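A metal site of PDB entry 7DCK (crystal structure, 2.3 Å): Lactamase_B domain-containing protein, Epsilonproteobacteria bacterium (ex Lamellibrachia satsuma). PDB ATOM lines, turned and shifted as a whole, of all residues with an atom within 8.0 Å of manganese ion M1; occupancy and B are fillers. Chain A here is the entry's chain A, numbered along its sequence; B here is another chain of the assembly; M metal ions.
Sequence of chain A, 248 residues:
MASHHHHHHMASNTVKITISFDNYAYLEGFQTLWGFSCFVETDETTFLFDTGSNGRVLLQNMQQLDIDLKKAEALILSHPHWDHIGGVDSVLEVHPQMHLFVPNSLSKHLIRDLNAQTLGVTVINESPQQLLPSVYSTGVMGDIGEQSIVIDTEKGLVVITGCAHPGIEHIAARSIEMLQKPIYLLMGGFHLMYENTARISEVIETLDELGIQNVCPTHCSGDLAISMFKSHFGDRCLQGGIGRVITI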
ATOM      1  N   ASN A  23      15.765 -19.120   1.123  1.00  0.00           N
ATOM      2  CA  ASN A  23      14.608 -18.470   1.714  1.00  0.00           C
ATOM      3  C   ASN A  23      13.292 -19.045   1.186  1.00  0.00           C
ATOM      4  O   ASN A  23      12.224 -18.575   1.584  1.00  0.00           O
ATOM      5  CB  ASN A  23      14.651 -16.947   1.504  1.00  0.00           C
ATOM      6  CG  ASN A  23      14.956 -16.562   0.074  1.00  0.00           C
ATOM      7  OD1 ASN A  23      16.112 -16.504  -0.329  1.00  0.00           O
ATOM      8  ND2 ASN A  23      13.914 -16.279  -0.688  1.00  0.00           N
ATOM      9  N   TRP A  34      17.188 -15.841   4.859  1.00  0.00           N
ATOM     10  CA  TRP A  34      17.754 -15.154   3.709  1.00  0.00           C
ATOM     11  C   TRP A  34      19.192 -15.609   3.462  1.00  0.00           C
ATOM     12  O   TRP A  34      20.072 -15.390   4.304  1.00  0.00           O
ATOM     13  CB  TRP A  34      17.720 -13.640   3.898  1.00  0.00           C
ATOM     14  CG  TRP A  34      18.000 -12.914   2.626  1.00  0.00           C
ATOM     15  CD1 TRP A  34      19.177 -12.332   2.258  1.00  0.00           C
ATOM     16  CD2 TRP A  34      17.096 -12.721   1.536  1.00  0.00           C
ATOM     17  NE1 TRP A  34      19.056 -11.769   1.010  1.00  0.00           N
ATOM     18  CE2 TRP A  34      17.783 -11.996   0.544  1.00  0.00           C
ATOM     19  CE3 TRP A  34      15.767 -13.074   1.301  1.00  0.00           C
ATOM     20  CZ2 TRP A  34      17.194 -11.619  -0.657  1.00  0.00           C
ATOM     21  CZ3 TRP A  34      15.183 -12.709   0.106  1.00  0.00           C
ATOM     22  CH2 TRP A  34      15.892 -11.985  -0.858  1.00  0.00           C
ATOM     23  N   GLY A  35      19.422 -16.234   2.316  1.00  0.00           N
ATOM     24  CA  GLY A  35      20.740 -16.712   1.960  1.00  0.00           C
ATOM     25  C   GLY A  35      20.630 -17.914   1.026  1.00  0.00           C
ATOM     26  O   GLY A  35      19.545 -18.315   0.624  1.00  0.00           O
ATOM     27  N   PHE A  36      21.792 -18.485   0.714  1.00  0.00           N
ATOM     28  CA  PHE A  36      21.857 -19.568  -0.246  1.00  0.00           C
ATOM     29  C   PHE A  36      23.026 -20.502   0.060  1.00  0.00           C
ATOM     30  O   PHE A  36      24.084 -20.052   0.484  1.00  0.00           O
ATOM     31  CB  PHE A  36      21.996 -19.037  -1.679  1.00  0.00           C
ATOM     32  CG  PHE A  36      21.818 -20.100  -2.723  1.00  0.00           C
ATOM     33  CD1 PHE A  36      20.623 -20.788  -2.826  1.00  0.00           C
ATOM     34  CD2 PHE A  36      22.848 -20.419  -3.588  1.00  0.00           C
ATOM     35  CE1 PHE A  36      20.446 -21.773  -3.774  1.00  0.00           C
ATOM     36  CE2 PHE A  36      22.684 -21.407  -4.539  1.00  0.00           C
ATOM     37  CZ  PHE A  36      21.480 -22.078  -4.635  1.00  0.00           C
ATOM     38  N   ASP A  50      28.807 -21.762  -1.346  1.00  0.00           N
ATOM     39  CA  ASP A  50      28.296 -20.797  -0.380  1.00  0.00           C
ATOM     40  C   ASP A  50      27.763 -21.489   0.871  1.00  0.00           C
ATOM     41  O   ASP A  50      27.617 -22.715   0.909  1.00  0.00           O
ATOM     42  CB  ASP A  50      27.222 -19.895  -1.006  1.00  0.00           C
ATOM     43  CG  ASP A  50      27.833 -18.812  -1.880  1.00  0.00           C
ATOM     44  OD1 ASP A  50      29.063 -18.624  -1.823  1.00  0.00           O
ATOM     45  OD2 ASP A  50      27.087 -18.143  -2.628  1.00  0.00           O
ATOM     46  N   SER A  78      30.802 -17.472  -3.439  1.00  0.00           N
ATOM     47  CA  SER A  78      30.494 -16.662  -4.615  1.00  0.00           C
ATOM     48  C   SER A  78      30.924 -15.217  -4.431  1.00  0.00           C
ATOM     49  O   SER A  78      31.540 -14.622  -5.331  1.00  0.00           O
ATOM     50  CB  SER A  78      28.993 -16.741  -4.922  1.00  0.00           C
ATOM     51  OG  SER A  78      28.228 -16.118  -3.907  1.00  0.00           O
ATOM     52  N   HIS A  79      30.615 -14.613  -3.280  1.00  0.00           N
ATOM     53  CA  HIS A  79      30.931 -13.216  -3.019  1.00  0.00           C
ATOM     54  C   HIS A  79      30.829 -12.907  -1.528  1.00  0.00           C
ATOM     55  O   HIS A  79      30.341 -13.760  -0.770  1.00  0.00           O
ATOM     56  CB  HIS A  79      30.027 -12.299  -3.874  1.00  0.00           C
ATOM     57  CG  HIS A  79      28.583 -12.300  -3.476  1.00  0.00           C
ATOM     58  ND1 HIS A  79      27.776 -13.410  -3.600  1.00  0.00           N
ATOM     59  CD2 HIS A  79      27.795 -11.309  -3.009  1.00  0.00           C
ATOM     60  CE1 HIS A  79      26.558 -13.107  -3.199  1.00  0.00           C
ATOM     61  NE2 HIS A  79      26.542 -11.838  -2.836  1.00  0.00           N
ATOM     62  N   HIS A  81      29.030 -11.301   0.654  1.00  0.00           N
ATOM     63  CA  HIS A  81      27.848 -10.830   1.364  1.00  0.00           C
ATOM     64  C   HIS A  81      27.490 -11.746   2.532  1.00  0.00           C
ATOM     65  O   HIS A  81      27.654 -12.973   2.454  1.00  0.00           O
ATOM     66  CB  HIS A  81      26.663 -10.691   0.407  1.00  0.00           C
ATOM     67  CG  HIS A  81      26.720  -9.456  -0.427  1.00  0.00           C
ATOM     68  ND1 HIS A  81      25.880  -9.234  -1.505  1.00  0.00           N
ATOM     69  CD2 HIS A  81      27.526  -8.361  -0.352  1.00  0.00           C
ATOM     70  CE1 HIS A  81      26.164  -8.066  -2.044  1.00  0.00           C
ATOM     71  NE2 HIS A  81      27.158  -7.509  -1.372  1.00  0.00           N
ATOM     72  N   TRP A  82      27.031 -11.132   3.624  1.00  0.00           N
ATOM     73  CA  TRP A  82      26.760 -11.831   4.873  1.00  0.00           C
ATOM     74  C   TRP A  82      25.923 -13.097   4.683  1.00  0.00           C
ATOM     75  O   TRP A  82      26.118 -14.091   5.395  1.00  0.00           O
ATOM     76  CB  TRP A  82      26.038 -10.893   5.841  1.00  0.00           C
ATOM     77  CG  TRP A  82      24.750 -10.385   5.260  1.00  0.00           C
ATOM     78  CD1 TRP A  82      24.588  -9.356   4.382  1.00  0.00           C
ATOM     79  CD2 TRP A  82      23.436 -10.932   5.479  1.00  0.00           C
ATOM     80  NE1 TRP A  82      23.255  -9.214   4.058  1.00  0.00           N
ATOM     81  CE2 TRP A  82      22.531 -10.170   4.717  1.00  0.00           C
ATOM     82  CE3 TRP A  82      22.942 -11.993   6.255  1.00  0.00           C
ATOM     83  CZ2 TRP A  82      21.156 -10.429   4.699  1.00  0.00           C
ATOM     84  CZ3 TRP A  82      21.576 -12.247   6.238  1.00  0.00           C
ATOM     85  CH2 TRP A  82      20.696 -11.468   5.468  1.00  0.00           C
ATOM     86  N   ASP A  83      24.989 -13.074   3.737  1.00  0.00           N
ATOM     87  CA  ASP A  83      24.075 -14.192   3.563  1.00  0.00           C
ATOM     88  C   ASP A  83      24.641 -15.289   2.678  1.00  0.00           C
ATOM     89  O   ASP A  83      23.903 -16.185   2.257  1.00  0.00           O
ATOM     90  CB  ASP A  83      22.744 -13.689   2.997  1.00  0.00           C
ATOM     91  CG  ASP A  83      22.909 -12.975   1.674  1.00  0.00           C
ATOM     92  OD1 ASP A  83      23.825 -12.125   1.561  1.00  0.00           O
ATOM     93  OD2 ASP A  83      22.138 -13.270   0.753  1.00  0.00           O
ATOM     94  N   HIS A  84      25.948 -15.246   2.374  1.00  0.00           N
ATOM     95  CA  HIS A  84      26.613 -16.333   1.683  1.00  0.00           C
ATOM     96  C   HIS A  84      27.850 -16.841   2.413  1.00  0.00           C
ATOM     97  O   HIS A  84      28.239 -17.993   2.198  1.00  0.00           O
ATOM     98  CB  HIS A  84      27.011 -15.911   0.253  1.00  0.00           C
ATOM     99  CG  HIS A  84      25.849 -15.519  -0.589  1.00  0.00           C
ATOM    100  ND1 HIS A  84      25.316 -16.336  -1.566  1.00  0.00           N
ATOM    101  CD2 HIS A  84      25.088 -14.394  -0.605  1.00  0.00           C
ATOM    102  CE1 HIS A  84      24.295 -15.736  -2.144  1.00  0.00           C
ATOM    103  NE2 HIS A  84      24.137 -14.554  -1.575  1.00  0.00           N
ATOM    104  N   GLU A 146      31.898 -10.838  -7.864  1.00  0.00           N
ATOM    105  CA  GLU A 146      31.215 -12.104  -7.645  1.00  0.00           C
ATOM    106  C   GLU A 146      31.637 -13.108  -8.709  1.00  0.00           C
ATOM    107  O   GLU A 146      31.684 -12.787  -9.905  1.00  0.00           O
ATOM    108  CB  GLU A 146      29.691 -11.922  -7.674  1.00  0.00           C
ATOM    109  CG  GLU A 146      28.923 -13.232  -7.589  1.00  0.00           C
ATOM    110  CD  GLU A 146      27.422 -13.050  -7.589  1.00  0.00           C
ATOM    111  OE1 GLU A 146      26.954 -11.883  -7.572  1.00  0.00           O
ATOM    112  OE2 GLU A 146      26.694 -14.060  -7.601  1.00  0.00           O
ATOM    113  N   GLY A 162      25.336 -17.298  -6.961  1.00  0.00           N
ATOM    114  CA  GLY A 162      24.905 -16.864  -5.639  1.00  0.00           C
ATOM    115  C   GLY A 162      23.775 -15.850  -5.682  1.00  0.00           C
ATOM    116  O   GLY A 162      22.618 -16.199  -5.444  1.00  0.00           O
ATOM    117  N   CYS A 163      24.085 -14.577  -5.945  1.00  0.00           N
ATOM    118  CA  CYS A 163      23.068 -13.553  -6.143  1.00  0.00           C
ATOM    119  C   CYS A 163      23.128 -12.917  -7.523  1.00  0.00           C
ATOM    120  O   CYS A 163      22.165 -12.246  -7.899  1.00  0.00           O
ATOM    121  CB  CYS A 163      23.145 -12.451  -5.036  1.00  0.00           C
ATOM    122  SG  CYS A 163      21.523 -11.665  -4.425  1.00  0.00           S
ATOM    123  N   ALA A 164      24.173 -13.183  -8.327  1.00  0.00           N
ATOM    124  CA  ALA A 164      24.230 -12.757  -9.733  1.00  0.00           C
ATOM    125  C   ALA A 164      24.195 -11.239  -9.867  1.00  0.00           C
ATOM    126  O   ALA A 164      23.564 -10.694 -10.769  1.00  0.00           O
ATOM    127  CB  ALA A 164      23.111 -13.386 -10.575  1.00  0.00           C
ATOM    128  N   HIS A 165      24.899 -10.551  -8.968  1.00  0.00           N
ATOM    129  CA  HIS A 165      25.044  -9.103  -9.061  1.00  0.00           C
ATOM    130  C   HIS A 165      25.530  -8.616 -10.426  1.00  0.00           C
ATOM    131  O   HIS A 165      24.991  -7.604 -10.913  1.00  0.00           O
ATOM    132  CB  HIS A 165      25.974  -8.606  -7.946  1.00  0.00           C
ATOM    133  CG  HIS A 165      25.406  -8.762  -6.570  1.00  0.00           C
ATOM    134  ND1 HIS A 165      24.418  -7.930  -6.066  1.00  0.00           N
ATOM    135  CD2 HIS A 165      25.681  -9.648  -5.580  1.00  0.00           C
ATOM    136  CE1 HIS A 165      24.115  -8.304  -4.839  1.00  0.00           C
ATOM    137  NE2 HIS A 165      24.871  -9.333  -4.513  1.00  0.00           N
ATOM    138  N   GLY A 189      20.440 -17.520  -7.292  1.00  0.00           N
ATOM    139  CA  GLY A 189      19.783 -16.232  -7.197  1.00  0.00           C
ATOM    140  C   GLY A 189      20.125 -15.329  -8.357  1.00  0.00           C
ATOM    141  O   GLY A 189      21.309 -15.095  -8.632  1.00  0.00           O
ATOM    142  N   HIS A 191      19.009 -12.072  -8.738  1.00  0.00           N
ATOM    143  CA  HIS A 191      18.971 -10.651  -8.357  1.00  0.00           C
ATOM    144  C   HIS A 191      18.072  -9.827  -9.270  1.00  0.00           C
ATOM    145  O   HIS A 191      18.443  -8.763  -9.776  1.00  0.00           O
ATOM    146  CB  HIS A 191      20.383 -10.051  -8.344  1.00  0.00           C
ATOM    147  CG  HIS A 191      20.623  -9.114  -7.197  1.00  0.00           C
ATOM    148  ND1 HIS A 191      20.601  -9.514  -5.884  1.00  0.00           N
ATOM    149  CD2 HIS A 191      20.893  -7.785  -7.183  1.00  0.00           C
ATOM    150  CE1 HIS A 191      20.847  -8.476  -5.100  1.00  0.00           C
ATOM    151  NE2 HIS A 191      21.026  -7.415  -5.869  1.00  0.00           N
ATOM    152  N   HIS A 219      16.431 -17.936  -4.209  1.00  0.00           N
ATOM    153  CA  HIS A 219      17.099 -16.934  -3.367  1.00  0.00           C
ATOM    154  C   HIS A 219      16.653 -15.522  -3.714  1.00  0.00           C
ATOM    155  O   HIS A 219      15.478 -15.179  -3.531  1.00  0.00           O
ATOM    156  CB  HIS A 219      18.628 -17.098  -3.451  1.00  0.00           C
ATOM    157  CG  HIS A 219      19.390 -16.104  -2.616  1.00  0.00           C
ATOM    158  ND1 HIS A 219      18.966 -15.721  -1.359  1.00  0.00           N
ATOM    159  CD2 HIS A 219      20.504 -15.385  -2.878  1.00  0.00           C
ATOM    160  CE1 HIS A 219      19.803 -14.826  -0.878  1.00  0.00           C
ATOM    161  NE2 HIS A 219      20.745 -14.602  -1.769  1.00  0.00           N
ATOM    162  N   CYS A 220      17.561 -14.672  -4.227  1.00  0.00           N
ATOM    163  CA  CYS A 220      17.212 -13.262  -4.407  1.00  0.00           C
ATOM    164  C   CYS A 220      16.573 -12.953  -5.755  1.00  0.00           C
ATOM    165  O   CYS A 220      16.612 -11.819  -6.213  1.00  0.00           O
ATOM    166  CB  CYS A 220      18.451 -12.386  -4.161  1.00  0.00           C
ATOM    167  SG  CYS A 220      19.928 -12.659  -5.266  1.00  0.00           S
ATOM    168  N   HIS B 109      16.774  -7.775   5.440  1.00  0.00           N
ATOM    169  CA  HIS B 109      16.632  -9.225   5.488  1.00  0.00           C
ATOM    170  C   HIS B 109      17.216  -9.794   6.778  1.00  0.00           C
ATOM    171  O   HIS B 109      16.610 -10.672   7.405  1.00  0.00           O
ATOM    172  CB  HIS B 109      17.328  -9.856   4.285  1.00  0.00           C
ATOM    173  CG  HIS B 109      16.743  -9.457   2.962  1.00  0.00           C
ATOM    174  ND1 HIS B 109      15.511  -9.896   2.527  1.00  0.00           N
ATOM    175  CD2 HIS B 109      17.239  -8.668   1.983  1.00  0.00           C
ATOM    176  CE1 HIS B 109      15.265  -9.378   1.336  1.00  0.00           C
ATOM    177  NE2 HIS B 109      16.291  -8.637   0.978  1.00  0.00           N
HETATM  178 MN    MN M   1      22.424 -13.126  -1.385  1.00  0.00          MN
HETATM  179 MN    MN M   2      24.696 -10.610  -2.658  1.00  0.00          MN
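Manganese ion M1 is bound by OD2 of Asp 83 (2.2 Å), NE2 of His 84 (2.2 Å) and NE2 of His 219 (2.3 Å). Manganese ion M1 has three donor atoms within binding distance.
Merely in contact with manganese ion M1: Cys 163 (3.5 Å). Of the 21 residues printed, 4 come within 4 Å of manganese ion M1. The nearest printed residue that does not touch manganese ion M1 is Trp 34 (4.3 Å).
The side-chain carboxylate (OD2) of Asp 83 lies close to the indole nitrogen (NE1) of Trp 34, at 3.4 Å. The backbone carbonyl oxygen of Asp 83 is in hydrogen-bond range of the backbone NH of Phe 36 (3.5 Å). ND1 of His 84 is in hydrogen-bond range of OD2 of Asp 50 (2.7 Å). The backbone carbonyl oxygen (O) of Gly 35 lies within hydrogen-bond range of a ring nitrogen (ND1) of His 219. The side-chain amide oxygen (OD1) of Asn 23 lies within hydrogen-bond range of a ring nitrogen (ND1) of His 219 (3.1 Å). SG of Cys 163 forms a disulfide with SG of Cys 220, at 2.1 Å. SG of Cys 163 is in hydrogen-bond range of ND1 of His 191 (2.8 Å). OE2 of Glu 146 sits at hydrogen-bond distance from N of Cys 163.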
